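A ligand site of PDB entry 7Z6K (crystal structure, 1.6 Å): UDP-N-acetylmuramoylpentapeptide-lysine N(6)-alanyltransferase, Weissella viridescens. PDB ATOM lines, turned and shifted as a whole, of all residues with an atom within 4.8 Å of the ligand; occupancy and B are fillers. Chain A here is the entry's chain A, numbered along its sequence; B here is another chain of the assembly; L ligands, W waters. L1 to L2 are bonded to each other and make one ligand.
The backbone NH (N) of Ala 1 of chain B lies within hydrogen-bond range of the side-chain hydroxyl (OG1) of Thr 210, at 3.0 Å.
NZ of Lys 37 is in salt-bridge range of OXT of DAL 5 of chain B, 2.7 Å away.
NH2 of Arg 212 is in hydrogen-bond range of O of DAL 4 of chain B.
The side-chain hydroxyl (OH) of Tyr 216 lies within hydrogen-bond range of the side-chain amino group (NZ) of Lys 37 (2.9 Å).
OG1 of Thr 210 sits at hydrogen-bond distance from N of FGA 2 of chain B, at 2.8 Å.
OXT of DAL 5 of chain B lies within salt-bridge range of the guanidinium group (NH2) of Arg 212, 3.3 Å away.
Merely in contact with the ligand: Phe 71, Ile 143, Thr 210, DAL 4 of chain B, Thr 65, His 211 and Cys 3 of chain B.
Hydrophobic or aromatic side chains within 4 Å of the ligand: Trp 40, Phe 71, Tyr 104, Ile 143 and Ala 1 of chain B.
Of the 20 residues printed, 15 come within 4 Å of the ligand.
The side-chain hydroxyl (OH) of Tyr 104 lies within hydrogen-bond range of an oxygen (O2) of LG2 L2, at 2.6 Å.
N of FGA 2 of chain B sits close to an oxygen (O7) of LIG L1, 3.4 Å away.
The backbone NH (N) of Ala 1 of chain B is bonded to a carbon (C10) of LIG L1, 1.4 Å away.
An oxygen (O10) of LG2 L2 is in salt-bridge range of the side-chain amino group (NZ) of Lys 37 (2.8 Å).
An oxygen (O1) of LG2 L2 sits at hydrogen-bond distance from the guanidinium group (NH1) of Arg 107 (3.2 Å).
The side-chain amide nitrogen (ND2) of Asn 39 lies within hydrogen-bond range of an oxygen (O11) of LG2 L2 (3.0 Å).
The guanidinium group (NH2) of Arg 212 is in salt-bridge range of an oxygen (O8) of LG2 L2.
The indole nitrogen of Trp 40 lies within hydrogen-bond range of an oxygen (O11) of LG2 L2, 2.9 Å away.
Water W8 lies within hydrogen-bond range of an oxygen (O7) of LIG L1 (2.5 Å), the backbone NH of Cys 3 of chain B (2.7 Å) and O of DAL 4 of chain B (2.9 Å).
Water W4 lies within hydrogen-bond range of OXT of DAL 5 of chain B (2.6 Å), an oxygen (O7) of LG2 L2 (2.7 Å) and the side-chain amino group (NZ) of Lys 37 (3.4 Å).
Water W2 bridges OD1 of Asn 39 and O10 of LG2 L2.
Water W3 bridges the guanidinium group (NH1) of Arg 212 (2.9 Å) and an oxygen (O3) of LIG L1 (3.0 Å).
Water W6 bridges the backbone NH (N) of Ala 1 of chain B (3.1 Å) and an oxygen (O2) of LIG L1 (3.1 Å).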
ATOM      1  N   LYS A  37       5.596 -28.782   7.734  1.00  0.00           N
ATOM      2  CA  LYS A  37       5.553 -27.761   6.676  1.00  0.00           C
ATOM      3  C   LYS A  37       4.424 -28.098   5.704  1.00  0.00           C
ATOM      4  O   LYS A  37       4.629 -28.262   4.506  1.00  0.00           O
ATOM      5  CB  LYS A  37       6.885 -27.688   5.946  1.00  0.00           C
ATOM      6  CG  LYS A  37       8.106 -27.441   6.849  1.00  0.00           C
ATOM      7  CD  LYS A  37       8.237 -25.975   7.224  1.00  0.00           C
ATOM      8  CE  LYS A  37       9.522 -25.712   7.995  1.00  0.00           C
ATOM      9  NZ  LYS A  37       9.428 -24.422   8.724  1.00  0.00           N
ATOM     10  N   ASN A  39       2.181 -26.443   4.342  1.00  0.00           N
ATOM     11  CA  ASN A  39       1.957 -25.474   3.282  1.00  0.00           C
ATOM     12  C   ASN A  39       3.004 -25.543   2.174  1.00  0.00           C
ATOM     13  O   ASN A  39       2.962 -24.720   1.250  1.00  0.00           O
ATOM     14  CB  ASN A  39       1.891 -24.064   3.882  1.00  0.00           C
ATOM     15  CG  ASN A  39       3.103 -23.737   4.742  1.00  0.00           C
ATOM     16  OD1 ASN A  39       3.666 -24.600   5.431  1.00  0.00           O
ATOM     17  ND2 ASN A  39       3.509 -22.467   4.725  1.00  0.00           N
ATOM     18  N   TRP A  40       3.925 -26.499   2.236  1.00  0.00           N
ATOM     19  CA  TRP A  40       4.927 -26.733   1.197  1.00  0.00           C
ATOM     20  C   TRP A  40       4.621 -28.046   0.493  1.00  0.00           C
ATOM     21  O   TRP A  40       3.941 -28.928   1.034  1.00  0.00           O
ATOM     22  CB  TRP A  40       6.337 -26.786   1.803  1.00  0.00           C
ATOM     23  CG  TRP A  40       6.801 -25.469   2.378  1.00  0.00           C
ATOM     24  CD1 TRP A  40       6.263 -24.795   3.452  1.00  0.00           C
ATOM     25  CD2 TRP A  40       7.926 -24.694   1.950  1.00  0.00           C
ATOM     26  NE1 TRP A  40       6.966 -23.642   3.684  1.00  0.00           N
ATOM     27  CE2 TRP A  40       7.991 -23.555   2.769  1.00  0.00           C
ATOM     28  CE3 TRP A  40       8.869 -24.845   0.917  1.00  0.00           C
ATOM     29  CZ2 TRP A  40       8.970 -22.576   2.613  1.00  0.00           C
ATOM     30  CZ3 TRP A  40       9.840 -23.860   0.765  1.00  0.00           C
ATOM     31  CH2 TRP A  40       9.887 -22.746   1.604  1.00  0.00           C
ATOM     32  N   ASP A  64       6.096 -21.340  -2.809  1.00  0.00           N
ATOM     33  CA  ASP A  64       5.764 -20.343  -3.810  1.00  0.00           C
ATOM     34  C   ASP A  64       6.691 -19.133  -3.715  1.00  0.00           C
ATOM     35  O   ASP A  64       7.359 -18.912  -2.702  1.00  0.00           O
ATOM     36  CB  ASP A  64       4.297 -19.919  -3.682  1.00  0.00           C
ATOM     37  CG  ASP A  64       3.336 -21.031  -4.076  1.00  0.00           C
ATOM     38  OD1 ASP A  64       2.434 -21.364  -3.286  1.00  0.00           O
ATOM     39  OD2 ASP A  64       3.505 -21.591  -5.186  1.00  0.00           O
ATOM     40  N   THR A  65       6.770 -18.398  -4.812  1.00  0.00           N
ATOM     41  CA  THR A  65       7.531 -17.165  -4.961  1.00  0.00           C
ATOM     42  C   THR A  65       6.636 -16.153  -5.648  1.00  0.00           C
ATOM     43  O   THR A  65       5.550 -16.498  -6.132  1.00  0.00           O
ATOM     44  CB  THR A  65       8.798 -17.387  -5.806  1.00  0.00           C
ATOM     45  OG1 THR A  65       8.429 -17.537  -7.177  1.00  0.00           O
ATOM     46  CG2 THR A  65       9.567 -18.613  -5.348  1.00  0.00           C
ATOM     47  N   PHE A  71      10.371 -22.401  -5.254  1.00  0.00           N
ATOM     48  CA  PHE A  71      11.618 -22.455  -4.505  1.00  0.00           C
ATOM     49  C   PHE A  71      11.730 -23.858  -3.911  1.00  0.00           C
ATOM     50  O   PHE A  71      10.876 -24.256  -3.119  1.00  0.00           O
ATOM     51  CB  PHE A  71      11.593 -21.383  -3.399  1.00  0.00           C
ATOM     52  CG  PHE A  71      12.712 -21.478  -2.399  1.00  0.00           C
ATOM     53  CD1 PHE A  71      14.025 -21.318  -2.804  1.00  0.00           C
ATOM     54  CD2 PHE A  71      12.440 -21.682  -1.046  1.00  0.00           C
ATOM     55  CE1 PHE A  71      15.074 -21.389  -1.884  1.00  0.00           C
ATOM     56  CE2 PHE A  71      13.483 -21.751  -0.114  1.00  0.00           C
ATOM     57  CZ  PHE A  71      14.810 -21.609  -0.548  1.00  0.00           C
ATOM     58  N   TYR A 104      13.129 -22.603  -9.620  1.00  0.00           N
ATOM     59  CA  TYR A 104      14.248 -21.798 -10.103  1.00  0.00           C
ATOM     60  C   TYR A 104      15.569 -22.176  -9.452  1.00  0.00           C
ATOM     61  O   TYR A 104      16.629 -21.827  -9.984  1.00  0.00           O
ATOM     62  CB  TYR A 104      13.976 -20.307  -9.893  1.00  0.00           C
ATOM     63  CG  TYR A 104      14.171 -19.768  -8.487  1.00  0.00           C
ATOM     64  CD1 TYR A 104      13.111 -19.761  -7.582  1.00  0.00           C
ATOM     65  CD2 TYR A 104      15.378 -19.198  -8.091  1.00  0.00           C
ATOM     66  CE1 TYR A 104      13.253 -19.240  -6.303  1.00  0.00           C
ATOM     67  CE2 TYR A 104      15.550 -18.672  -6.808  1.00  0.00           C
ATOM     68  CZ  TYR A 104      14.474 -18.702  -5.918  1.00  0.00           C
ATOM     69  OH  TYR A 104      14.605 -18.185  -4.659  1.00  0.00           O
ATOM     70  N   ARG A 107      18.002 -25.440  -3.190  1.00  0.00           N
ATOM     71  CA  ARG A 107      18.882 -25.013  -2.115  1.00  0.00           C
ATOM     72  C   ARG A 107      18.957 -26.101  -1.061  1.00  0.00           C
ATOM     73  O   ARG A 107      17.930 -26.674  -0.688  1.00  0.00           O
ATOM     74  CB  ARG A 107      18.373 -23.719  -1.457  1.00  0.00           C
ATOM     75  CG  ARG A 107      19.131 -23.333  -0.207  1.00  0.00           C
ATOM     76  CD  ARG A 107      18.753 -21.930   0.226  1.00  0.00           C
ATOM     77  NE  ARG A 107      19.205 -20.951  -0.750  1.00  0.00           N
ATOM     78  CZ  ARG A 107      18.771 -19.697  -0.817  1.00  0.00           C
ATOM     79  NH1 ARG A 107      17.892 -19.224   0.061  1.00  0.00           N
ATOM     80  NH2 ARG A 107      19.240 -18.907  -1.778  1.00  0.00           N
ATOM     81  N   ILE A 143      18.601 -18.850   5.487  1.00  0.00           N
ATOM     82  CA  ILE A 143      17.370 -19.311   6.126  1.00  0.00           C
ATOM     83  C   ILE A 143      17.658 -19.856   7.525  1.00  0.00           C
ATOM     84  O   ILE A 143      17.042 -19.435   8.508  1.00  0.00           O
ATOM     85  CB  ILE A 143      16.665 -20.355   5.248  1.00  0.00           C
ATOM     86  CG1 ILE A 143      16.261 -19.729   3.902  1.00  0.00           C
ATOM     87  CG2 ILE A 143      15.454 -20.904   5.968  1.00  0.00           C
ATOM     88  CD1 ILE A 143      15.773 -20.746   2.882  1.00  0.00           C
ATOM     89  N   THR A 210       8.340 -12.414  15.590  1.00  0.00           N
ATOM     90  CA  THR A 210       7.276 -13.203  14.994  1.00  0.00           C
ATOM     91  C   THR A 210       7.274 -14.615  15.566  1.00  0.00           C
ATOM     92  O   THR A 210       8.307 -15.131  15.999  1.00  0.00           O
ATOM     93  CB  THR A 210       7.435 -13.248  13.464  1.00  0.00           C
ATOM     94  OG1 THR A 210       8.711 -13.800  13.125  1.00  0.00           O
ATOM     95  CG2 THR A 210       7.326 -11.847  12.879  1.00  0.00           C
ATOM     96  N   HIS A 211       6.089 -15.234  15.578  1.00  0.00           N
ATOM     97  CA  HIS A 211       5.909 -16.529  16.240  1.00  0.00           C
ATOM     98  C   HIS A 211       4.893 -17.374  15.488  1.00  0.00           C
ATOM     99  O   HIS A 211       3.921 -16.875  14.905  1.00  0.00           O
ATOM    100  CB  HIS A 211       5.481 -16.335  17.690  1.00  0.00           C
ATOM    101  CG  HIS A 211       4.199 -15.579  17.845  1.00  0.00           C
ATOM    102  ND1 HIS A 211       2.985 -16.205  18.088  1.00  0.00           N
ATOM    103  CD2 HIS A 211       3.927 -14.260  17.746  1.00  0.00           C
ATOM    104  CE1 HIS A 211       2.037 -15.288  18.163  1.00  0.00           C
ATOM    105  NE2 HIS A 211       2.585 -14.095  17.948  1.00  0.00           N
ATOM    106  N   ARG A 212       5.121 -18.687  15.537  1.00  0.00           N
ATOM    107  CA  ARG A 212       4.334 -19.664  14.805  1.00  0.00           C
ATOM    108  C   ARG A 212       3.041 -20.009  15.544  1.00  0.00           C
ATOM    109  O   ARG A 212       2.988 -19.966  16.775  1.00  0.00           O
ATOM    110  CB  ARG A 212       5.158 -20.932  14.586  1.00  0.00           C
ATOM    111  CG  ARG A 212       6.478 -20.664  13.875  1.00  0.00           C
ATOM    112  CD  ARG A 212       7.042 -21.952  13.341  1.00  0.00           C
ATOM    113  NE  ARG A 212       8.331 -21.785  12.668  1.00  0.00           N
ATOM    114  CZ  ARG A 212       8.474 -21.678  11.350  1.00  0.00           C
ATOM    115  NH1 ARG A 212       7.419 -21.623  10.557  1.00  0.00           N
ATOM    116  NH2 ARG A 212       9.691 -21.617  10.832  1.00  0.00           N
ATOM    117  N   PRO A 213       1.973 -20.327  14.804  1.00  0.00           N
ATOM    118  CA  PRO A 213       0.723 -20.753  15.437  1.00  0.00           C
ATOM    119  C   PRO A 213       0.859 -22.114  16.087  1.00  0.00           C
ATOM    120  O   PRO A 213       1.773 -22.903  15.786  1.00  0.00           O
ATOM    121  CB  PRO A 213      -0.291 -20.760  14.275  1.00  0.00           C
ATOM    122  CG  PRO A 213       0.541 -20.983  13.054  1.00  0.00           C
ATOM    123  CD  PRO A 213       1.883 -20.326  13.325  1.00  0.00           C
ATOM    124  N   TYR A 216       1.247 -25.477  14.161  1.00  0.00           N
ATOM    125  CA  TYR A 216       2.573 -25.899  13.700  1.00  0.00           C
ATOM    126  C   TYR A 216       3.153 -26.953  14.638  1.00  0.00           C
ATOM    127  O   TYR A 216       3.636 -28.007  14.194  1.00  0.00           O
ATOM    128  CB  TYR A 216       3.489 -24.673  13.632  1.00  0.00           C
ATOM    129  CG  TYR A 216       4.853 -24.887  13.028  1.00  0.00           C
ATOM    130  CD1 TYR A 216       5.048 -24.775  11.653  1.00  0.00           C
ATOM    131  CD2 TYR A 216       5.941 -25.199  13.825  1.00  0.00           C
ATOM    132  CE1 TYR A 216       6.289 -24.949  11.083  1.00  0.00           C
ATOM    133  CE2 TYR A 216       7.192 -25.404  13.266  1.00  0.00           C
ATOM    134  CZ  TYR A 216       7.361 -25.265  11.906  1.00  0.00           C
ATOM    135  OH  TYR A 216       8.599 -25.461  11.331  1.00  0.00           O
ATOM    136  N   LEU A 333      15.565 -12.960  -7.385  1.00  0.00           N
ATOM    137  CA  LEU A 333      15.101 -13.292  -6.039  1.00  0.00           C
ATOM    138  C   LEU A 333      16.202 -13.496  -5.017  1.00  0.00           C
ATOM    139  O   LEU A 333      15.901 -13.532  -3.818  1.00  0.00           O
ATOM    140  CB  LEU A 333      14.236 -14.555  -6.090  1.00  0.00           C
ATOM    141  CG  LEU A 333      12.983 -14.467  -6.957  1.00  0.00           C
ATOM    142  CD1 LEU A 333      12.167 -15.757  -6.859  1.00  0.00           C
ATOM    143  CD2 LEU A 333      12.149 -13.252  -6.514  1.00  0.00           C
ATOM    144  N   ALA B   1       9.549 -15.507  10.780  1.00  0.00           N
ATOM    145  CA  ALA B   1      10.720 -14.870  10.189  1.00  0.00           C
ATOM    146  C   ALA B   1      11.793 -14.586  11.249  1.00  0.00           C
ATOM    147  O   ALA B   1      12.990 -14.535  10.927  1.00  0.00           O
ATOM    148  CB  ALA B   1      10.325 -13.578   9.467  1.00  0.00           C
ATOM    149  N   FGA B   2      11.374 -14.421  12.498  1.00  0.00           N
ATOM    150  CA  FGA B   2      12.308 -14.111  13.573  1.00  0.00           C
ATOM    151  C   FGA B   2      12.128 -12.690  14.006  1.00  0.00           C
ATOM    152  O   FGA B   2      11.028 -12.141  13.920  1.00  0.00           O
ATOM    153  CB  FGA B   2      12.054 -15.025  14.774  1.00  0.00           C
ATOM    154  CG  FGA B   2      12.195 -16.496  14.404  1.00  0.00           C
ATOM    155  CD  FGA B   2      13.644 -16.936  14.544  1.00  0.00           C
ATOM    156  OE1 FGA B   2      14.558 -16.132  14.451  1.00  0.00           O
ATOM    157  OXT FGA B   2      13.158 -12.006  14.524  1.00  0.00           O
ATOM    158  N   CYS B   3      13.677 -18.231  13.938  1.00  0.00           N
ATOM    159  CA  CYS B   3      15.054 -18.729  13.818  1.00  0.00           C
ATOM    160  C   CYS B   3      15.089 -19.961  12.927  1.00  0.00           C
ATOM    161  O   CYS B   3      15.642 -21.013  13.308  1.00  0.00           O
ATOM    162  CB  CYS B   3      15.622 -19.046  15.202  1.00  0.00           C
ATOM    163  SG  CYS B   3      17.434 -19.059  15.274  1.00  0.00           S
ATOM    164  N   DAL B   4      14.507 -19.836  11.748  1.00  0.00           N
ATOM    165  CA  DAL B   4      14.308 -20.969  10.841  1.00  0.00           C
ATOM    166  CB  DAL B   4      13.587 -20.505   9.590  1.00  0.00           C
ATOM    167  C   DAL B   4      13.512 -22.059  11.548  1.00  0.00           C
ATOM    168  O   DAL B   4      12.487 -21.764  12.191  1.00  0.00           O
ATOM    169  N   DAL B   5      13.986 -23.304  11.435  1.00  0.00           N
ATOM    170  CA  DAL B   5      13.307 -24.430  12.089  1.00  0.00           C
ATOM    171  CB  DAL B   5      14.067 -25.717  11.862  1.00  0.00           C
ATOM    172  C   DAL B   5      11.864 -24.551  11.589  1.00  0.00           C
ATOM    173  O   DAL B   5      10.943 -24.847  12.372  1.00  0.00           O
ATOM    174  OXT DAL B   5      11.578 -24.327  10.412  1.00  0.00           O
HETATM  175  C1  LIG L   1       7.026 -19.014   7.256  1.00  0.00           C
HETATM  176  C2  LIG L   1       7.664 -18.092   8.295  1.00  0.00           C
HETATM  177  C3  LIG L   1       6.932 -18.221   9.628  1.00  0.00           C
HETATM  178  C4  LIG L   1       5.431 -18.065   9.446  1.00  0.00           C
HETATM  179  C5  LIG L   1       4.888 -18.959   8.333  1.00  0.00           C
HETATM  180  C6  LIG L   1       3.437 -18.650   8.024  1.00  0.00           C
HETATM  181  C7  LIG L   1      10.028 -17.555   7.987  1.00  0.00           C
HETATM  182  C8  LIG L   1      11.440 -18.019   8.132  1.00  0.00           C
HETATM  183  C9  LIG L   1       8.364 -17.570  11.473  1.00  0.00           C
HETATM  184  C10 LIG L   1       9.693 -16.840  11.264  1.00  0.00           C
HETATM  185  C11 LIG L   1       7.773 -17.257  12.839  1.00  0.00           C
HETATM  186  O1  LIG L   1       7.220 -20.338   7.643  1.00  0.00           O
HETATM  187  O2  LIG L   1       7.396 -17.180  10.500  1.00  0.00           O
HETATM  188  O3  LIG L   1       4.732 -18.395  10.648  1.00  0.00           O
HETATM  189  O4  LIG L   1       5.636 -18.730   7.126  1.00  0.00           O
HETATM  190  O5  LIG L   1       2.858 -19.593   7.123  1.00  0.00           O
HETATM  191  O6  LIG L   1       9.758 -16.460   7.482  1.00  0.00           O
HETATM  192  O7  LIG L   1      10.748 -17.526  11.320  1.00  0.00           O
HETATM  193  N1  LIG L   1       9.078 -18.380   8.427  1.00  0.00           N
HETATM  194  N1  LG2 L   2      12.680 -18.330   0.825  1.00  0.00           N
HETATM  195  C1  LG2 L   2      13.832 -18.122   0.095  1.00  0.00           C
HETATM  196  N2  LG2 L   2      13.654 -18.061  -1.270  1.00  0.00           N
HETATM  197  C2  LG2 L   2      12.465 -18.188  -1.950  1.00  0.00           C
HETATM  198  C3  LG2 L   2      11.304 -18.397  -1.122  1.00  0.00           C
HETATM  199  C4  LG2 L   2      11.453 -18.451   0.221  1.00  0.00           C
HETATM  200  O1  LG2 L   2      14.936 -17.990   0.598  1.00  0.00           O
HETATM  201  O2  LG2 L   2      12.463 -18.126  -3.195  1.00  0.00           O
HETATM  202  C5  LG2 L   2      12.821 -18.362   2.293  1.00  0.00           C
HETATM  203  C6  LG2 L   2      11.837 -17.474   3.044  1.00  0.00           C
HETATM  204  O3  LG2 L   2      12.215 -16.100   2.964  1.00  0.00           O
HETATM  205  C7  LG2 L   2      11.960 -18.069   4.447  1.00  0.00           C
HETATM  206  C8  LG2 L   2      12.224 -19.563   4.165  1.00  0.00           C
HETATM  207  O4  LG2 L   2      12.531 -19.660   2.761  1.00  0.00           O
HETATM  208  O5  LG2 L   2      13.093 -17.566   5.137  1.00  0.00           O
HETATM  209  C9  LG2 L   2      11.114 -20.510   4.547  1.00  0.00           C
HETATM  210  O6  LG2 L   2      11.062 -20.490   5.987  1.00  0.00           O
HETATM  211  P1  LG2 L   2      10.202 -21.535   6.797  1.00  0.00           P
HETATM  212  O7  LG2 L   2      10.826 -22.867   6.578  1.00  0.00           O
HETATM  213  O8  LG2 L   2      10.008 -21.074   8.244  1.00  0.00           O
HETATM  214  O9  LG2 L   2       8.768 -21.486   6.112  1.00  0.00           O
HETATM  215  P2  LG2 L   2       7.316 -21.608   6.747  1.00  0.00           P
HETATM  216  O10 LG2 L   2       7.387 -22.871   7.600  1.00  0.00           O
HETATM  217  O11 LG2 L   2       6.257 -21.676   5.680  1.00  0.00           O
HETATM  218  O   HOH W   1      15.545 -15.728   3.459  1.00  0.00           O
HETATM  219  O   HOH W   2       4.916 -24.066   7.792  1.00  0.00           O
HETATM  220  O   HOH W   3       4.622 -21.330  11.155  1.00  0.00           O
HETATM  221  O   HOH W   4      12.783 -23.874   8.166  1.00  0.00           O
HETATM  222  O   HOH W   5      10.862 -15.518  -3.063  1.00  0.00           O
HETATM  223  O   HOH W   6       6.957 -14.190   9.652  1.00  0.00           O
HETATM  224  O   HOH W   7      10.564 -24.654   4.616  1.00  0.00           O
HETATM  225  O   HOH W   8      11.347 -19.254  13.095  1.00  0.00           O
HETATM  226  O   HOH W   9       8.544 -16.318  -1.390  1.00  0.00           O
HETATM  227  O   HOH W  10       6.342 -19.670   3.752  1.00  0.00           O
HETATM  228  O   HOH W  11      13.721 -14.878   0.290  1.00  0.00           O
